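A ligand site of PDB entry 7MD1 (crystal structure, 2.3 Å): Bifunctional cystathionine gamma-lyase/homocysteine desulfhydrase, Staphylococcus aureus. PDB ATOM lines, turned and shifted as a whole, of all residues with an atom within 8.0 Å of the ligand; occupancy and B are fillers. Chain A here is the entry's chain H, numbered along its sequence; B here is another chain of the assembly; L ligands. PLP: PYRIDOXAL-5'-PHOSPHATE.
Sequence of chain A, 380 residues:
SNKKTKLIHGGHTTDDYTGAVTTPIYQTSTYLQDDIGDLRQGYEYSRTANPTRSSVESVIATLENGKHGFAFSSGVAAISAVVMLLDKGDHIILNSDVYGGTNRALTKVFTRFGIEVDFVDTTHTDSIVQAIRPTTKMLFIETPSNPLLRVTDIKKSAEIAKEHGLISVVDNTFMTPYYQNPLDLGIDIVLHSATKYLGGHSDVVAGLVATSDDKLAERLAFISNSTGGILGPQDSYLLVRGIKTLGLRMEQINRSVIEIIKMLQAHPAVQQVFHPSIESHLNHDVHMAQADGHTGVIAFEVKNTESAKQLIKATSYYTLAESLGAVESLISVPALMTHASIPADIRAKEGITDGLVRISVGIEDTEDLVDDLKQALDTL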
ATOM      1  N   SER A   1      -8.535  20.524 -14.797  1.00  0.00           N
ATOM      2  CA  SER A   1      -9.915  20.057 -14.780  1.00  0.00           C
ATOM      3  C   SER A   1      -9.988  18.635 -14.231  1.00  0.00           C
ATOM      4  O   SER A   1     -10.016  18.441 -13.021  1.00  0.00           O
ATOM      5  CB  SER A   1     -10.532  20.102 -16.181  1.00  0.00           C
ATOM      6  OG  SER A   1     -11.932  19.924 -16.132  1.00  0.00           O
ATOM      7  N   ASN A   2     -10.012  17.634 -15.107  1.00  0.00           N
ATOM      8  CA  ASN A   2     -10.086  16.256 -14.655  1.00  0.00           C
ATOM      9  C   ASN A   2      -8.739  15.774 -14.112  1.00  0.00           C
ATOM     10  O   ASN A   2      -7.698  16.408 -14.299  1.00  0.00           O
ATOM     11  CB  ASN A   2     -10.582  15.378 -15.795  1.00  0.00           C
ATOM     12  CG  ASN A   2     -12.061  15.582 -16.083  1.00  0.00           C
ATOM     13  OD1 ASN A   2     -12.796  16.077 -15.219  1.00  0.00           O
ATOM     14  ND2 ASN A   2     -12.503  15.210 -17.271  1.00  0.00           N
ATOM     15  N   LYS A   3      -8.771  14.639 -13.405  1.00  0.00           N
ATOM     16  CA  LYS A   3      -7.637  14.200 -12.596  1.00  0.00           C
ATOM     17  C   LYS A   3      -6.384  13.925 -13.440  1.00  0.00           C
ATOM     18  O   LYS A   3      -5.269  14.311 -13.066  1.00  0.00           O
ATOM     19  CB  LYS A   3      -8.012  12.946 -11.806  1.00  0.00           C
ATOM     20  CG  LYS A   3      -9.272  13.059 -10.988  1.00  0.00           C
ATOM     21  CD  LYS A   3      -9.363  11.916  -9.953  1.00  0.00           C
ATOM     22  CE  LYS A   3      -9.827  10.590 -10.588  1.00  0.00           C
ATOM     23  NZ  LYS A   3     -10.160   9.557  -9.542  1.00  0.00           N
ATOM     24  N   LYS A   4      -6.549  13.227 -14.565  1.00  0.00           N
ATOM     25  CA  LYS A   4      -5.386  12.928 -15.395  1.00  0.00           C
ATOM     26  C   LYS A   4      -4.733  14.193 -15.938  1.00  0.00           C
ATOM     27  O   LYS A   4      -3.522  14.207 -16.178  1.00  0.00           O
ATOM     28  CB  LYS A   4      -5.773  12.006 -16.539  1.00  0.00           C
ATOM     29  CG  LYS A   4      -6.067  10.584 -16.104  1.00  0.00           C
ATOM     30  CD  LYS A   4      -6.432   9.761 -17.330  1.00  0.00           C
ATOM     31  CE  LYS A   4      -6.837   8.367 -16.943  1.00  0.00           C
ATOM     32  NZ  LYS A   4      -7.361   7.605 -18.097  1.00  0.00           N
ATOM     33  N   THR A   5      -5.517  15.252 -16.137  1.00  0.00           N
ATOM     34  CA  THR A   5      -4.962  16.523 -16.596  1.00  0.00           C
ATOM     35  C   THR A   5      -4.241  17.222 -15.460  1.00  0.00           C
ATOM     36  O   THR A   5      -3.146  17.773 -15.657  1.00  0.00           O
ATOM     37  CB  THR A   5      -6.096  17.394 -17.142  1.00  0.00           C
ATOM     38  OG1 THR A   5      -6.795  16.669 -18.144  1.00  0.00           O
ATOM     39  CG2 THR A   5      -5.582  18.710 -17.722  1.00  0.00           C
ATOM     40  N   LYS A   6      -4.838  17.194 -14.273  1.00  0.00           N
ATOM     41  CA  LYS A   6      -4.251  17.786 -13.090  1.00  0.00           C
ATOM     42  C   LYS A   6      -2.891  17.165 -12.768  1.00  0.00           C
ATOM     43  O   LYS A   6      -1.975  17.854 -12.304  1.00  0.00           O
ATOM     44  CB  LYS A   6      -5.218  17.619 -11.912  1.00  0.00           C
ATOM     45  CG  LYS A   6      -4.915  18.439 -10.685  1.00  0.00           C
ATOM     46  CD  LYS A   6      -6.052  18.252  -9.666  1.00  0.00           C
ATOM     47  CE  LYS A   6      -5.772  18.937  -8.345  1.00  0.00           C
ATOM     48  NZ  LYS A   6      -6.788  18.609  -7.312  1.00  0.00           N
ATOM     49  N   LEU A   7      -2.736  15.853 -13.003  1.00  0.00           N
ATOM     50  CA  LEU A   7      -1.443  15.231 -12.765  1.00  0.00           C
ATOM     51  C   LEU A   7      -0.360  15.813 -13.662  1.00  0.00           C
ATOM     52  O   LEU A   7       0.811  15.885 -13.255  1.00  0.00           O
ATOM     53  CB  LEU A   7      -1.514  13.715 -12.979  1.00  0.00           C
ATOM     54  CG  LEU A   7      -2.268  12.989 -11.884  1.00  0.00           C
ATOM     55  CD1 LEU A   7      -2.591  11.599 -12.375  1.00  0.00           C
ATOM     56  CD2 LEU A   7      -1.409  12.963 -10.636  1.00  0.00           C
ATOM     57  N   ILE A   8      -0.716  16.222 -14.870  1.00  0.00           N
ATOM     58  CA  ILE A   8       0.279  16.729 -15.803  1.00  0.00           C
ATOM     59  C   ILE A   8       0.546  18.210 -15.556  1.00  0.00           C
ATOM     60  O   ILE A   8       1.684  18.661 -15.555  1.00  0.00           O
ATOM     61  CB  ILE A   8      -0.166  16.468 -17.250  1.00  0.00           C
ATOM     62  CG1 ILE A   8      -0.421  14.966 -17.462  1.00  0.00           C
ATOM     63  CG2 ILE A   8       0.881  16.977 -18.229  1.00  0.00           C
ATOM     64  CD1 ILE A   8       0.716  14.099 -16.957  1.00  0.00           C
ATOM     65  N   HIS A   9      -0.511  18.984 -15.314  1.00  0.00           N
ATOM     66  CA  HIS A   9      -0.364  20.427 -15.293  1.00  0.00           C
ATOM     67  C   HIS A   9      -0.436  21.070 -13.916  1.00  0.00           C
ATOM     68  O   HIS A   9      -0.084  22.240 -13.783  1.00  0.00           O
ATOM     69  CB  HIS A   9      -1.419  21.044 -16.221  1.00  0.00           C
ATOM     70  CG  HIS A   9      -1.205  20.686 -17.661  1.00  0.00           C
ATOM     71  ND1 HIS A   9      -0.247  21.295 -18.432  1.00  0.00           N
ATOM     72  CD2 HIS A   9      -1.776  19.747 -18.443  1.00  0.00           C
ATOM     73  CE1 HIS A   9      -0.257  20.764 -19.640  1.00  0.00           C
ATOM     74  NE2 HIS A   9      -1.187  19.818 -19.676  1.00  0.00           N
ATOM     75  N   GLY A  10      -0.824  20.324 -12.880  1.00  0.00           N
ATOM     76  CA  GLY A  10      -0.881  20.884 -11.536  1.00  0.00           C
ATOM     77  C   GLY A  10       0.492  20.996 -10.897  1.00  0.00           C
ATOM     78  O   GLY A  10       1.385  20.190 -11.127  1.00  0.00           O
ATOM     79  N   GLY A  11       0.653  22.023 -10.062  1.00  0.00           N
ATOM     80  CA  GLY A  11       1.945  22.293  -9.457  1.00  0.00           C
ATOM     81  C   GLY A  11       2.854  23.038 -10.418  1.00  0.00           C
ATOM     82  O   GLY A  11       2.543  23.273 -11.582  1.00  0.00           O
ATOM     83  N   THR A  62      -0.983  20.467  -4.468  1.00  0.00           N
ATOM     84  CA  THR A  62      -2.037  20.574  -5.477  1.00  0.00           C
ATOM     85  C   THR A  62      -2.876  19.307  -5.562  1.00  0.00           C
ATOM     86  O   THR A  62      -4.108  19.371  -5.617  1.00  0.00           O
ATOM     87  CB  THR A  62      -1.427  20.899  -6.852  1.00  0.00           C
ATOM     88  OG1 THR A  62      -0.837  22.197  -6.828  1.00  0.00           O
ATOM     89  CG2 THR A  62      -2.484  20.847  -7.929  1.00  0.00           C
ATOM     90  N   LEU A  63      -2.220  18.138  -5.610  1.00  0.00           N
ATOM     91  CA  LEU A  63      -2.965  16.894  -5.824  1.00  0.00           C
ATOM     92  C   LEU A  63      -3.893  16.574  -4.657  1.00  0.00           C
ATOM     93  O   LEU A  63      -4.952  15.961  -4.866  1.00  0.00           O
ATOM     94  CB  LEU A  63      -1.992  15.736  -6.085  1.00  0.00           C
ATOM     95  CG  LEU A  63      -1.130  15.831  -7.347  1.00  0.00           C
ATOM     96  CD1 LEU A  63      -0.280  14.577  -7.506  1.00  0.00           C
ATOM     97  CD2 LEU A  63      -1.998  16.050  -8.575  1.00  0.00           C
ATOM     98  N   GLU A  64      -3.533  16.971  -3.434  1.00  0.00           N
ATOM     99  CA  GLU A  64      -4.371  16.752  -2.264  1.00  0.00           C
ATOM    100  C   GLU A  64      -5.259  17.950  -1.945  1.00  0.00           C
ATOM    101  O   GLU A  64      -5.884  17.972  -0.875  1.00  0.00           O
ATOM    102  CB  GLU A  64      -3.510  16.412  -1.032  1.00  0.00           C
ATOM    103  CG  GLU A  64      -2.807  15.050  -1.076  1.00  0.00           C
ATOM    104  CD  GLU A  64      -3.751  13.823  -0.861  1.00  0.00           C
ATOM    105  OE1 GLU A  64      -4.984  13.955  -1.014  1.00  0.00           O
ATOM    106  OE2 GLU A  64      -3.230  12.716  -0.566  1.00  0.00           O
ATOM    107  N   ASN A  65      -5.330  18.955  -2.837  1.00  0.00           N
ATOM    108  CA  ASN A  65      -6.106  20.184  -2.588  1.00  0.00           C
ATOM    109  C   ASN A  65      -5.747  20.841  -1.262  1.00  0.00           C
ATOM    110  O   ASN A  65      -6.609  21.361  -0.545  1.00  0.00           O
ATOM    111  CB  ASN A  65      -7.608  19.914  -2.662  1.00  0.00           C
ATOM    112  CG  ASN A  65      -8.026  19.357  -4.003  1.00  0.00           C
ATOM    113  OD1 ASN A  65      -7.615  19.856  -5.050  1.00  0.00           O
ATOM    114  ND2 ASN A  65      -8.835  18.299  -3.983  1.00  0.00           N
ATOM    115  N   ASN A 181      -8.977  11.898  -1.073  1.00  0.00           N
ATOM    116  CA  ASN A 181      -8.419  13.203  -0.670  1.00  0.00           C
ATOM    117  C   ASN A 181      -8.900  13.566   0.724  1.00  0.00           C
ATOM    118  O   ASN A 181      -9.914  14.260   0.889  1.00  0.00           O
ATOM    119  CB  ASN A 181      -8.764  14.282  -1.685  1.00  0.00           C
ATOM    120  CG  ASN A 181      -8.292  13.937  -3.095  1.00  0.00           C
ATOM    121  OD1 ASN A 181      -9.091  13.769  -3.998  1.00  0.00           O
ATOM    122  ND2 ASN A 181      -6.984  13.817  -3.276  1.00  0.00           N
ATOM    123  N   ASP A 184     -10.060  17.162   1.735  1.00  0.00           N
ATOM    124  CA  ASP A 184     -11.395  17.549   1.285  1.00  0.00           C
ATOM    125  C   ASP A 184     -12.470  17.099   2.263  1.00  0.00           C
ATOM    126  O   ASP A 184     -13.604  17.558   2.168  1.00  0.00           O
ATOM    127  CB  ASP A 184     -11.702  16.939  -0.080  1.00  0.00           C
ATOM    128  CG  ASP A 184     -11.056  17.714  -1.233  1.00  0.00           C
ATOM    129  OD1 ASP A 184     -10.513  18.821  -0.994  1.00  0.00           O
ATOM    130  OD2 ASP A 184     -11.082  17.195  -2.375  1.00  0.00           O
ATOM    131  N   SER B 316      -5.572  25.811 -23.390  1.00  0.00           N
ATOM    132  CA  SER B 316      -5.008  25.755 -22.058  1.00  0.00           C
ATOM    133  C   SER B 316      -4.056  24.589 -21.862  1.00  0.00           C
ATOM    134  O   SER B 316      -3.077  24.719 -21.120  1.00  0.00           O
ATOM    135  CB  SER B 316      -6.127  25.681 -21.017  1.00  0.00           C
ATOM    136  OG  SER B 316      -6.900  26.872 -21.040  1.00  0.00           O
ATOM    137  N   TYR B 317      -4.290  23.454 -22.516  1.00  0.00           N
ATOM    138  CA  TYR B 317      -3.546  22.228 -22.259  1.00  0.00           C
ATOM    139  C   TYR B 317      -2.621  21.815 -23.402  1.00  0.00           C
ATOM    140  O   TYR B 317      -2.019  20.738 -23.325  1.00  0.00           O
ATOM    141  CB  TYR B 317      -4.523  21.096 -21.943  1.00  0.00           C
ATOM    142  CG  TYR B 317      -5.486  21.464 -20.830  1.00  0.00           C
ATOM    143  CD1 TYR B 317      -5.006  21.938 -19.624  1.00  0.00           C
ATOM    144  CD2 TYR B 317      -6.859  21.365 -21.007  1.00  0.00           C
ATOM    145  CE1 TYR B 317      -5.868  22.300 -18.606  1.00  0.00           C
ATOM    146  CE2 TYR B 317      -7.737  21.723 -19.983  1.00  0.00           C
ATOM    147  CZ  TYR B 317      -7.233  22.197 -18.780  1.00  0.00           C
ATOM    148  OH  TYR B 317      -8.056  22.558 -17.737  1.00  0.00           O
ATOM    149  N   GLU B 364      -2.990  13.711 -20.822  1.00  0.00           N
ATOM    150  CA  GLU B 364      -4.065  14.384 -20.108  1.00  0.00           C
ATOM    151  C   GLU B 364      -5.395  13.676 -20.368  1.00  0.00           C
ATOM    152  O   GLU B 364      -5.515  12.800 -21.218  1.00  0.00           O
ATOM    153  CB  GLU B 364      -4.191  15.847 -20.534  1.00  0.00           C
ATOM    154  CG  GLU B 364      -2.963  16.664 -20.291  1.00  0.00           C
ATOM    155  CD  GLU B 364      -2.072  16.786 -21.523  1.00  0.00           C
ATOM    156  OE1 GLU B 364      -2.152  15.915 -22.412  1.00  0.00           O
ATOM    157  OE2 GLU B 364      -1.301  17.779 -21.605  1.00  0.00           O
ATOM    158  N   ASP B 368     -10.794  16.585 -21.518  1.00  0.00           N
ATOM    159  CA  ASP B 368     -10.159  17.898 -21.427  1.00  0.00           C
ATOM    160  C   ASP B 368      -9.424  18.263 -22.722  1.00  0.00           C
ATOM    161  O   ASP B 368      -9.509  19.416 -23.172  1.00  0.00           O
ATOM    162  CB  ASP B 368      -9.197  17.930 -20.244  1.00  0.00           C
ATOM    163  CG  ASP B 368      -9.917  17.947 -18.910  1.00  0.00           C
ATOM    164  OD1 ASP B 368     -11.052  18.466 -18.840  1.00  0.00           O
ATOM    165  OD2 ASP B 368      -9.338  17.429 -17.930  1.00  0.00           O
HETATM  166  N1  PLP L   1      -5.385  22.728 -10.978  1.00  0.00           N
HETATM  167  C2  PLP L   1      -4.968  22.413 -12.217  1.00  0.00           C
HETATM  168  C2A PLP L   1      -3.619  22.890 -12.676  1.00  0.00           C
HETATM  169  C3  PLP L   1      -5.773  21.666 -13.052  1.00  0.00           C
HETATM  170  O3  PLP L   1      -5.337  21.355 -14.306  1.00  0.00           O
HETATM  171  C4  PLP L   1      -7.030  21.226 -12.628  1.00  0.00           C
HETATM  172  C4A PLP L   1      -7.915  20.434 -13.509  1.00  0.00           C
HETATM  173  C5  PLP L   1      -7.452  21.570 -11.329  1.00  0.00           C
HETATM  174  C6  PLP L   1      -6.591  22.318 -10.549  1.00  0.00           C
HETATM  175  C5A PLP L   1      -8.798  21.137 -10.776  1.00  0.00           C
HETATM  176  O4P PLP L   1      -8.781  21.031  -9.356  1.00  0.00           O
HETATM  177  P   PLP L   1     -10.041  20.363  -8.596  1.00  0.00           P
HETATM  178  O1P PLP L   1     -10.236  21.038  -7.260  1.00  0.00           O
HETATM  179  O2P PLP L   1     -11.255  20.546  -9.471  1.00  0.00           O
HETATM  180  O3P PLP L   1      -9.808  18.883  -8.398  1.00  0.00           O
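N of Ser 1 is covalently linked to C4A of the ligand (1.4 Å).
The side-chain amino group of Lys 6 is in salt-bridge range of an oxygen (O3P) of the ligand, at 3.2 Å.
OG of Ser 1 sits close to OD1 of Asp 368 of chain B (3.2 Å).
The side-chain amide oxygen (OD1) of Asn 65 lies within hydrogen-bond range of the side-chain amino group (NZ) of Lys 6, 2.7 Å away.
NZ of Lys 6 sits close to O of Thr 62 (3.3 Å).
ND2 of Asn 65 is in hydrogen-bond range of OD2 of Asp 184 (3.0 Å).
A ring nitrogen (NE2) of His 9 lies within hydrogen-bond range of the side-chain carboxylate (OE2) of Glu 364 of chain B, 2.8 Å away.
OD2 of Asp 368 of chain B lies within hydrogen-bond range of N of Asn 2, 2.9 Å away.
Merely in contact with the ligand: Asn 2, His 9, Gly 10 and Asn 65.
Of the 21 residues printed, 6 come within 4 Å of the ligand.
Along chain A the residues within 4 Å of the ligand span positions 1 to 65.
The nearest printed residue that does not touch the ligand is Thr 5 (4.3 Å).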
